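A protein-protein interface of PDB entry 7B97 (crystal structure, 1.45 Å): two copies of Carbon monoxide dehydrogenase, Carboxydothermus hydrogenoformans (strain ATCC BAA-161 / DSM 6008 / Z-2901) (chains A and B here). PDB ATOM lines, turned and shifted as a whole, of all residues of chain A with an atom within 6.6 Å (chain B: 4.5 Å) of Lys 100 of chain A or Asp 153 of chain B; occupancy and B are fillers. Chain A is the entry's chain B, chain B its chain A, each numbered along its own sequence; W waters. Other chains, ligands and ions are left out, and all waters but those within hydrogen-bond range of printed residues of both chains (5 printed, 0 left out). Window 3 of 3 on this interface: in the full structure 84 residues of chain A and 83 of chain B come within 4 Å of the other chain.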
ATOM      1  N   ALA A  95      12.343  28.840 -20.871  1.00  0.00           N
ATOM      2  CA  ALA A  95      12.997  27.541 -20.882  1.00  0.00           C
ATOM      3  C   ALA A  95      12.231  26.538 -20.028  1.00  0.00           C
ATOM      4  O   ALA A  95      11.990  25.408 -20.453  1.00  0.00           O
ATOM      5  CB  ALA A  95      14.441  27.667 -20.402  1.00  0.00           C
ATOM      6  N   TYR A  96      11.871  26.925 -18.802  1.00  0.00           N
ATOM      7  CA  TYR A  96      11.142  26.017 -17.933  1.00  0.00           C
ATOM      8  C   TYR A  96       9.851  25.556 -18.593  1.00  0.00           C
ATOM      9  O   TYR A  96       9.512  24.368 -18.537  1.00  0.00           O
ATOM     10  CB  TYR A  96      10.856  26.722 -16.601  1.00  0.00           C
ATOM     11  CG  TYR A  96      10.320  25.806 -15.530  1.00  0.00           C
ATOM     12  CD1 TYR A  96      11.140  24.906 -14.904  1.00  0.00           C
ATOM     13  CD2 TYR A  96       8.978  25.841 -15.171  1.00  0.00           C
ATOM     14  CE1 TYR A  96      10.655  24.046 -13.948  1.00  0.00           C
ATOM     15  CE2 TYR A  96       8.478  24.998 -14.185  1.00  0.00           C
ATOM     16  CZ  TYR A  96       9.341  24.106 -13.578  1.00  0.00           C
ATOM     17  OH  TYR A  96       8.900  23.249 -12.596  1.00  0.00           O
ATOM     18  N   GLU A  97       9.120  26.475 -19.230  1.00  0.00           N
ATOM     19  CA  GLU A  97       7.872  26.087 -19.895  1.00  0.00           C
ATOM     20  C   GLU A  97       8.143  25.172 -21.082  1.00  0.00           C
ATOM     21  O   GLU A  97       7.370  24.243 -21.329  1.00  0.00           O
ATOM     22  CB  GLU A  97       7.064  27.311 -20.315  1.00  0.00           C
ATOM     23  CG  GLU A  97       6.602  28.139 -19.139  1.00  0.00           C
ATOM     24  CD  GLU A  97       5.258  28.807 -19.345  1.00  0.00           C
ATOM     25  OE1 GLU A  97       4.947  29.173 -20.488  1.00  0.00           O
ATOM     26  OE2 GLU A  97       4.550  29.012 -18.338  1.00  0.00           O
ATOM     27  N   ALA A  98       9.239  25.388 -21.813  1.00  0.00           N
ATOM     28  CA  ALA A  98       9.593  24.463 -22.888  1.00  0.00           C
ATOM     29  C   ALA A  98       9.838  23.056 -22.349  1.00  0.00           C
ATOM     30  O   ALA A  98       9.407  22.070 -22.956  1.00  0.00           O
ATOM     31  CB  ALA A  98      10.840  24.972 -23.636  1.00  0.00           C
ATOM     32  N   TYR A  99      10.566  22.947 -21.234  1.00  0.00           N
ATOM     33  CA  TYR A  99      10.896  21.636 -20.681  1.00  0.00           C
ATOM     34  C   TYR A  99       9.661  20.950 -20.138  1.00  0.00           C
ATOM     35  O   TYR A  99       9.474  19.739 -20.341  1.00  0.00           O
ATOM     36  CB  TYR A  99      11.958  21.782 -19.594  1.00  0.00           C
ATOM     37  CG  TYR A  99      13.208  22.521 -20.067  1.00  0.00           C
ATOM     38  CD1 TYR A  99      13.582  22.521 -21.408  1.00  0.00           C
ATOM     39  CD2 TYR A  99      14.011  23.206 -19.172  1.00  0.00           C
ATOM     40  CE1 TYR A  99      14.741  23.206 -21.851  1.00  0.00           C
ATOM     41  CE2 TYR A  99      15.157  23.883 -19.580  1.00  0.00           C
ATOM     42  CZ  TYR A  99      15.510  23.888 -20.925  1.00  0.00           C
ATOM     43  OH  TYR A  99      16.641  24.538 -21.352  1.00  0.00           O
ATOM     44  N   LYS A 100       8.802  21.697 -19.446  1.00  0.00           N
ATOM     45  CA  LYS A 100       7.546  21.104 -18.991  1.00  0.00           C
ATOM     46  C   LYS A 100       6.669  20.716 -20.163  1.00  0.00           C
ATOM     47  O   LYS A 100       5.959  19.704 -20.087  1.00  0.00           O
ATOM     48  CB  LYS A 100       6.814  22.043 -18.030  1.00  0.00           C
ATOM     49  CG  LYS A 100       7.562  22.249 -16.705  1.00  0.00           C
ATOM     50  CD  LYS A 100       6.817  21.789 -15.477  1.00  0.00           C
ATOM     51  CE  LYS A 100       5.507  22.542 -15.296  1.00  0.00           C
ATOM     52  NZ  LYS A 100       4.881  22.281 -13.982  1.00  0.00           N
ATOM     53  N   THR A 101       6.727  21.479 -21.264  1.00  0.00           N
ATOM     54  CA  THR A 101       5.926  21.141 -22.433  1.00  0.00           C
ATOM     55  C   THR A 101       6.450  19.872 -23.097  1.00  0.00           C
ATOM     56  O   THR A 101       5.665  19.005 -23.508  1.00  0.00           O
ATOM     57  CB  THR A 101       5.906  22.299 -23.424  1.00  0.00           C
ATOM     58  OG1 THR A 101       5.257  23.422 -22.829  1.00  0.00           O
ATOM     59  CG2 THR A 101       5.158  21.885 -24.675  1.00  0.00           C
ATOM     60  N   LEU A 102       7.769  19.704 -23.157  1.00  0.00           N
ATOM     61  CA  LEU A 102       8.304  18.461 -23.722  1.00  0.00           C
ATOM     62  C   LEU A 102       7.903  17.266 -22.869  1.00  0.00           C
ATOM     63  O   LEU A 102       7.467  16.238 -23.390  1.00  0.00           O
ATOM     64  CB  LEU A 102       9.827  18.557 -23.887  1.00  0.00           C
ATOM     65  CG  LEU A 102      10.506  17.288 -24.402  1.00  0.00           C
ATOM     66  CD1 LEU A 102       9.969  16.875 -25.768  1.00  0.00           C
ATOM     67  CD2 LEU A 102      12.033  17.473 -24.487  1.00  0.00           C
ATOM     68  N   LYS A 103       8.050  17.384 -21.551  1.00  0.00           N
ATOM     69  CA  LYS A 103       7.675  16.292 -20.665  1.00  0.00           C
ATOM     70  C   LYS A 103       6.206  15.933 -20.838  1.00  0.00           C
ATOM     71  O   LYS A 103       5.865  14.765 -21.056  1.00  0.00           O
ATOM     72  CB  LYS A 103       8.000  16.682 -19.222  1.00  0.00           C
ATOM     73  CG  LYS A 103       7.854  15.509 -18.254  1.00  0.00           C
ATOM     74  CD  LYS A 103       7.987  15.950 -16.820  1.00  0.00           C
ATOM     75  CE  LYS A 103       9.422  15.930 -16.362  1.00  0.00           C
ATOM     76  NZ  LYS A 103       9.488  15.857 -14.868  1.00  0.00           N
ATOM     77  N   MET A 104       5.317  16.922 -20.781  1.00  0.00           N
ATOM     78  CA  MET A 104       3.895  16.595 -20.897  1.00  0.00           C
ATOM     79  C   MET A 104       3.511  16.124 -22.294  1.00  0.00           C
ATOM     80  O   MET A 104       2.529  15.378 -22.452  1.00  0.00           O
ATOM     81  CB  MET A 104       3.048  17.762 -20.380  1.00  0.00           C
ATOM     82  CG  MET A 104       3.318  18.036 -18.888  1.00  0.00           C
ATOM     83  SD  MET A 104       2.457  17.001 -17.735  1.00  0.00           S
ATOM     84  CE  MET A 104       1.051  16.728 -18.677  1.00  0.00           C
ATOM     85  N   THR A 105       4.249  16.553 -23.322  1.00  0.00           N
ATOM     86  CA  THR A 105       4.063  15.968 -24.643  1.00  0.00           C
ATOM     87  C   THR A 105       4.412  14.488 -24.635  1.00  0.00           C
ATOM     88  O   THR A 105       3.668  13.663 -25.184  1.00  0.00           O
ATOM     89  CB  THR A 105       4.898  16.730 -25.666  1.00  0.00           C
ATOM     90  OG1 THR A 105       4.384  18.053 -25.772  1.00  0.00           O
ATOM     91  CG2 THR A 105       4.821  16.072 -27.049  1.00  0.00           C
ATOM     92  N   THR A 110      -0.568  16.711 -24.614  1.00  0.00           N
ATOM     93  CA  THR A 110      -0.595  17.915 -25.431  1.00  0.00           C
ATOM     94  C   THR A 110      -0.963  17.541 -26.853  1.00  0.00           C
ATOM     95  O   THR A 110      -0.969  16.361 -27.212  1.00  0.00           O
ATOM     96  CB  THR A 110       0.770  18.620 -25.435  1.00  0.00           C
ATOM     97  OG1 THR A 110       1.662  17.901 -26.286  1.00  0.00           O
ATOM     98  CG2 THR A 110       1.351  18.707 -24.017  1.00  0.00           C
ATOM     99  N   SER A 143      14.233  16.405 -20.513  1.00  0.00           N
ATOM    100  CA  SER A 143      13.544  17.514 -19.860  1.00  0.00           C
ATOM    101  C   SER A 143      14.018  17.677 -18.424  1.00  0.00           C
ATOM    102  O   SER A 143      14.270  18.799 -17.971  1.00  0.00           O
ATOM    103  CB  SER A 143      12.034  17.276 -19.888  1.00  0.00           C
ATOM    104  OG  SER A 143      11.573  17.217 -21.225  1.00  0.00           O
ATOM    105  N   ILE A 147      15.958  20.877 -16.825  1.00  0.00           N
ATOM    106  CA  ILE A 147      15.474  21.528 -15.611  1.00  0.00           C
ATOM    107  C   ILE A 147      16.581  21.580 -14.559  1.00  0.00           C
ATOM    108  O   ILE A 147      16.771  22.597 -13.895  1.00  0.00           O
ATOM    109  CB  ILE A 147      14.194  20.840 -15.100  1.00  0.00           C
ATOM    110  CG1 ILE A 147      13.044  21.104 -16.071  1.00  0.00           C
ATOM    111  CG2 ILE A 147      13.864  21.292 -13.694  1.00  0.00           C
ATOM    112  CD1 ILE A 147      11.813  20.248 -15.836  1.00  0.00           C
ATOM    113  N   TYR A 151      18.346  24.764 -12.475  1.00  0.00           N
ATOM    114  CA  TYR A 151      18.299  24.776 -11.019  1.00  0.00           C
ATOM    115  C   TYR A 151      19.674  24.616 -10.371  1.00  0.00           C
ATOM    116  O   TYR A 151      19.776  24.734  -9.147  1.00  0.00           O
ATOM    117  CB  TYR A 151      17.432  23.598 -10.535  1.00  0.00           C
ATOM    118  CG  TYR A 151      15.922  23.709 -10.689  1.00  0.00           C
ATOM    119  CD1 TYR A 151      15.318  24.752 -11.375  1.00  0.00           C
ATOM    120  CD2 TYR A 151      15.118  22.731 -10.141  1.00  0.00           C
ATOM    121  CE1 TYR A 151      13.940  24.814 -11.485  1.00  0.00           C
ATOM    122  CE2 TYR A 151      13.770  22.778 -10.241  1.00  0.00           C
ATOM    123  CZ  TYR A 151      13.183  23.809 -10.905  1.00  0.00           C
ATOM    124  OH  TYR A 151      11.810  23.788 -10.966  1.00  0.00           O
ATOM    125  N   TYR A 372      -1.362  29.765 -19.810  1.00  0.00           N
ATOM    126  CA  TYR A 372      -0.886  28.543 -20.454  1.00  0.00           C
ATOM    127  C   TYR A 372      -0.502  27.459 -19.457  1.00  0.00           C
ATOM    128  O   TYR A 372       0.156  27.720 -18.447  1.00  0.00           O
ATOM    129  CB  TYR A 372       0.358  28.876 -21.275  1.00  0.00           C
ATOM    130  CG  TYR A 372       1.046  27.681 -21.890  1.00  0.00           C
ATOM    131  CD1 TYR A 372       0.549  27.100 -23.032  1.00  0.00           C
ATOM    132  CD2 TYR A 372       2.216  27.154 -21.348  1.00  0.00           C
ATOM    133  CE1 TYR A 372       1.147  26.028 -23.600  1.00  0.00           C
ATOM    134  CE2 TYR A 372       2.846  26.071 -21.937  1.00  0.00           C
ATOM    135  CZ  TYR A 372       2.294  25.503 -23.057  1.00  0.00           C
ATOM    136  OH  TYR A 372       2.877  24.418 -23.672  1.00  0.00           O
ATOM    137  N   PRO A 374       0.707  23.216 -20.433  1.00  0.00           N
ATOM    138  CA  PRO A 374       0.778  22.252 -21.555  1.00  0.00           C
ATOM    139  C   PRO A 374      -0.436  21.339 -21.692  1.00  0.00           C
ATOM    140  O   PRO A 374      -0.887  21.086 -22.816  1.00  0.00           O
ATOM    141  CB  PRO A 374       2.053  21.462 -21.247  1.00  0.00           C
ATOM    142  CG  PRO A 374       2.866  22.359 -20.370  1.00  0.00           C
ATOM    143  CD  PRO A 374       1.913  23.197 -19.595  1.00  0.00           C
ATOM    144  N   TYR B 151      12.132  25.607  -4.299  1.00  0.00           N
ATOM    145  CA  TYR B 151      12.150  25.341  -5.738  1.00  0.00           C
ATOM    146  C   TYR B 151      10.776  25.028  -6.317  1.00  0.00           C
ATOM    147  O   TYR B 151      10.663  24.875  -7.533  1.00  0.00           O
ATOM    148  CB  TYR B 151      13.030  24.128  -6.051  1.00  0.00           C
ATOM    149  CG  TYR B 151      14.518  24.364  -6.173  1.00  0.00           C
ATOM    150  CD1 TYR B 151      15.048  25.087  -7.211  1.00  0.00           C
ATOM    151  CD2 TYR B 151      15.391  23.800  -5.272  1.00  0.00           C
ATOM    152  CE1 TYR B 151      16.420  25.282  -7.332  1.00  0.00           C
ATOM    153  CE2 TYR B 151      16.748  23.987  -5.379  1.00  0.00           C
ATOM    154  CZ  TYR B 151      17.262  24.726  -6.410  1.00  0.00           C
ATOM    155  OH  TYR B 151      18.626  24.892  -6.506  1.00  0.00           O
ATOM    156  N   ARG B 152       9.743  24.925  -5.484  1.00  0.00           N
ATOM    157  CA  ARG B 152       8.405  24.555  -5.942  1.00  0.00           C
ATOM    158  C   ARG B 152       7.906  25.535  -7.007  1.00  0.00           C
ATOM    159  O   ARG B 152       8.023  26.748  -6.851  1.00  0.00           O
ATOM    160  CB  ARG B 152       7.488  24.563  -4.702  1.00  0.00           C
ATOM    161  CG  ARG B 152       6.226  23.751  -4.730  1.00  0.00           C
ATOM    162  CD  ARG B 152       5.544  23.798  -3.352  1.00  0.00           C
ATOM    163  NE  ARG B 152       5.532  25.128  -2.737  1.00  0.00           N
ATOM    164  CZ  ARG B 152       4.739  26.125  -3.129  1.00  0.00           C
ATOM    165  NH1 ARG B 152       3.889  25.947  -4.130  1.00  0.00           N
ATOM    166  NH2 ARG B 152       4.791  27.305  -2.523  1.00  0.00           N
ATOM    167  N   ASP B 153       7.338  25.001  -8.099  1.00  0.00           N
ATOM    168  CA  ASP B 153       6.761  25.863  -9.132  1.00  0.00           C
ATOM    169  C   ASP B 153       5.306  26.238  -8.826  1.00  0.00           C
ATOM    170  O   ASP B 153       4.712  25.794  -7.851  1.00  0.00           O
ATOM    171  CB  ASP B 153       6.969  25.293 -10.551  1.00  0.00           C
ATOM    172  CG  ASP B 153       6.086  24.101 -10.889  1.00  0.00           C
ATOM    173  OD1 ASP B 153       5.050  23.856 -10.234  1.00  0.00           O
ATOM    174  OD2 ASP B 153       6.431  23.433 -11.897  1.00  0.00           O
ATOM    175  N   TYR B 154       4.748  27.127  -9.654  1.00  0.00           N
ATOM    176  CA  TYR B 154       3.470  27.731  -9.294  1.00  0.00           C
ATOM    177  C   TYR B 154       2.348  26.720  -9.265  1.00  0.00           C
ATOM    178  O   TYR B 154       1.280  27.030  -8.721  1.00  0.00           O
ATOM    179  CB  TYR B 154       3.089  28.860 -10.262  1.00  0.00           C
ATOM    180  CG  TYR B 154       2.408  28.356 -11.501  1.00  0.00           C
ATOM    181  CD1 TYR B 154       3.149  27.758 -12.509  1.00  0.00           C
ATOM    182  CD2 TYR B 154       1.023  28.443 -11.657  1.00  0.00           C
ATOM    183  CE1 TYR B 154       2.550  27.274 -13.641  1.00  0.00           C
ATOM    184  CE2 TYR B 154       0.414  27.954 -12.783  1.00  0.00           C
ATOM    185  CZ  TYR B 154       1.186  27.366 -13.775  1.00  0.00           C
ATOM    186  OH  TYR B 154       0.610  26.872 -14.920  1.00  0.00           O
ATOM    187  N   ASP B 155       2.564  25.529  -9.824  1.00  0.00           N
ATOM    188  CA  ASP B 155       1.517  24.522  -9.984  1.00  0.00           C
ATOM    189  C   ASP B 155       1.671  23.327  -9.049  1.00  0.00           C
ATOM    190  O   ASP B 155       0.920  22.354  -9.184  1.00  0.00           O
ATOM    191  CB  ASP B 155       1.483  24.049 -11.443  1.00  0.00           C
ATOM    192  CG  ASP B 155       0.129  23.542 -11.868  1.00  0.00           C
ATOM    193  OD1 ASP B 155      -0.897  24.164 -11.500  1.00  0.00           O
ATOM    194  OD2 ASP B 155       0.106  22.526 -12.593  1.00  0.00           O
ATOM    195  N   GLU B 156       2.599  23.374  -8.101  1.00  0.00           N
ATOM    196  CA  GLU B 156       2.780  22.310  -7.118  1.00  0.00           C
ATOM    197  C   GLU B 156       2.452  22.845  -5.726  1.00  0.00           C
ATOM    198  O   GLU B 156       3.029  23.864  -5.311  1.00  0.00           O
ATOM    199  CB  GLU B 156       4.250  21.805  -7.160  1.00  0.00           C
ATOM    200  CG  GLU B 156       4.554  20.608  -6.250  1.00  0.00           C
ATOM    201  CD  GLU B 156       5.955  20.009  -6.475  1.00  0.00           C
ATOM    202  OE1 GLU B 156       6.832  20.686  -7.065  1.00  0.00           O
ATOM    203  OE2 GLU B 156       6.178  18.849  -6.044  1.00  0.00           O
ATOM    204  N   ALA B 181       3.919  30.210  -5.796  1.00  0.00           N
ATOM    205  CA  ALA B 181       4.954  29.226  -6.031  1.00  0.00           C
ATOM    206  C   ALA B 181       5.995  29.323  -4.920  1.00  0.00           C
ATOM    207  O   ALA B 181       5.912  30.169  -4.020  1.00  0.00           O
ATOM    208  CB  ALA B 181       5.621  29.504  -7.376  1.00  0.00           C
ATOM    209  N   HIS B 185      10.825  30.429  -8.052  1.00  0.00           N
ATOM    210  CA  HIS B 185       9.963  30.654  -9.209  1.00  0.00           C
ATOM    211  C   HIS B 185       9.160  31.934  -9.073  1.00  0.00           C
ATOM    212  O   HIS B 185       8.972  32.657 -10.063  1.00  0.00           O
ATOM    213  CB  HIS B 185       9.018  29.477  -9.407  1.00  0.00           C
ATOM    214  CG  HIS B 185       9.597  28.370 -10.217  1.00  0.00           C
ATOM    215  ND1 HIS B 185       9.669  28.412 -11.593  1.00  0.00           N
ATOM    216  CD2 HIS B 185      10.168  27.201  -9.842  1.00  0.00           C
ATOM    217  CE1 HIS B 185      10.211  27.289 -12.027  1.00  0.00           C
ATOM    218  NE2 HIS B 185      10.551  26.555 -10.983  1.00  0.00           N
HETATM  219  O   HOH W   1      20.214  22.799  -6.995  1.00  0.00           O
HETATM  220  O   HOH W   2       1.953  22.976 -14.559  1.00  0.00           O
HETATM  221  O   HOH W   3      10.352  22.386  -9.157  1.00  0.00           O
HETATM  222  O   HOH W   4       2.369  27.984 -17.090  1.00  0.00           O
HETATM  223  O   HOH W   5      -1.516  28.293 -15.734  1.00  0.00           O
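Of the 8 printed residues of chain B, 4 touch a printed residue of chain A.
Of the 17 printed residues of chain A, 4 touch a printed residue of chain B.
Printed residues of chain A that touch a printed residue of chain B: Tyr 96, Lys 100, Tyr 151 and Tyr 372.
Hydrophobic or aromatic side chains of chain A that line the printed part of chain B: Tyr 96 and Tyr 151.
Along chain A the printed residues that touch a printed residue of chain B span positions 96 to 372.
Lys 100 of chain A touches just one residue of chain B: Asp 153 (2.8 Å).
Of the printed residues of chain B, Tyr 151 of chain A touches Tyr 151 (2.9 Å) and His 185 (3.0 Å).
Printed residues of chain B within 4 Å of Tyr 372 of chain A: Tyr 154 (3.7 Å).
Printed residues of chain A within 4 Å of Tyr 151 of chain B: Tyr 151 (2.9 Å).
Printed residues of chain A within 4 Å of Tyr 154 of chain B: Tyr 372.
Of the printed residues of chain A, His 185 of chain B touches Tyr 96 (3.6 Å) and Tyr 151 (3.0 Å).
The nearest printed residue of chain B that does not touch Lys 100 of chain A is Asp 155 of chain B (4.6 Å).
The nearest printed residue of chain A that does not touch Asp 153 of chain B is Tyr 151 of chain A (5.1 Å).
The nearest printed residue of chain A that does not touch His 185 of chain B is Ile 147 of chain A (6.8 Å).
A ring nitrogen (NE2) of His 185 of chain B sits at hydrogen-bond distance from the side-chain hydroxyl of Tyr 151 of chain A.
The side-chain hydroxyl of Tyr 151 of chain B lies within hydrogen-bond range of the backbone carbonyl oxygen of Tyr 151 of chain A (2.9 Å).
The side-chain hydroxyl (OH) of Tyr 96 of chain A is in hydrogen-bond range of the side-chain carboxylate (OD2) of Asp 153 of chain B (2.6 Å).
The side-chain amino group of Lys 100 of chain A lies within salt-bridge range of the side-chain carboxylate of Asp 153 of chain B.
The side-chain hydroxyl (OH) of Tyr 96 of chain A sits close to the side-chain hydroxyl (OH) of Tyr 151 of chain A (3.4 Å).
The side-chain carboxylate (OD1) of Asp 153 of chain B sits at hydrogen-bond distance from the backbone NH (N) of Glu 156 of chain B (3.3 Å).
The side-chain hydroxyl (OG1) of Thr 101 of chain A is in hydrogen-bond range of the side-chain hydroxyl (OH) of Tyr 372 of chain A (2.7 Å).
OD1 of Asp 153 of chain B sits close to N of Asp 155 of chain B, at 3.0 Å.
Tyr 151 of chain B touches its own counterpart, Tyr 151 of chain A.
1 position is printed for both chains.
Of the 6 pairs that touch across the chains among the printed residues, 1 has its exchanged pair printed and touching as well.
Among the printed residues, merely in contact across the chains: Tyr 96 of chain A with His 185 of chain B and Tyr 372 of chain A with Tyr 154 of chain B.
Water W4 lies within hydrogen-bond range of O of Tyr 372 of chain A (2.6 Å), OE2 of Glu 97 of chain A (2.7 Å) and OH of Tyr 154 of chain B (3.0 Å).
Water W1 lies within hydrogen-bond range of the side-chain hydroxyl (OH) of Tyr 151 of chain B (2.7 Å) and the backbone carbonyl oxygen (O) of Tyr 151 of chain A (2.9 Å).
Water W5 lies within hydrogen-bond range of OH of Tyr 154 of chain B and O of Tyr 372 of chain A.
Water W3 lies within hydrogen-bond range of OH of Tyr 151 of chain A (2.7 Å) and O of Tyr 151 of chain B (3.0 Å).
Water W2 lies within hydrogen-bond range of the side-chain carboxylate of Asp 155 of chain B and the side-chain amino group of Lys 100 of chain A.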
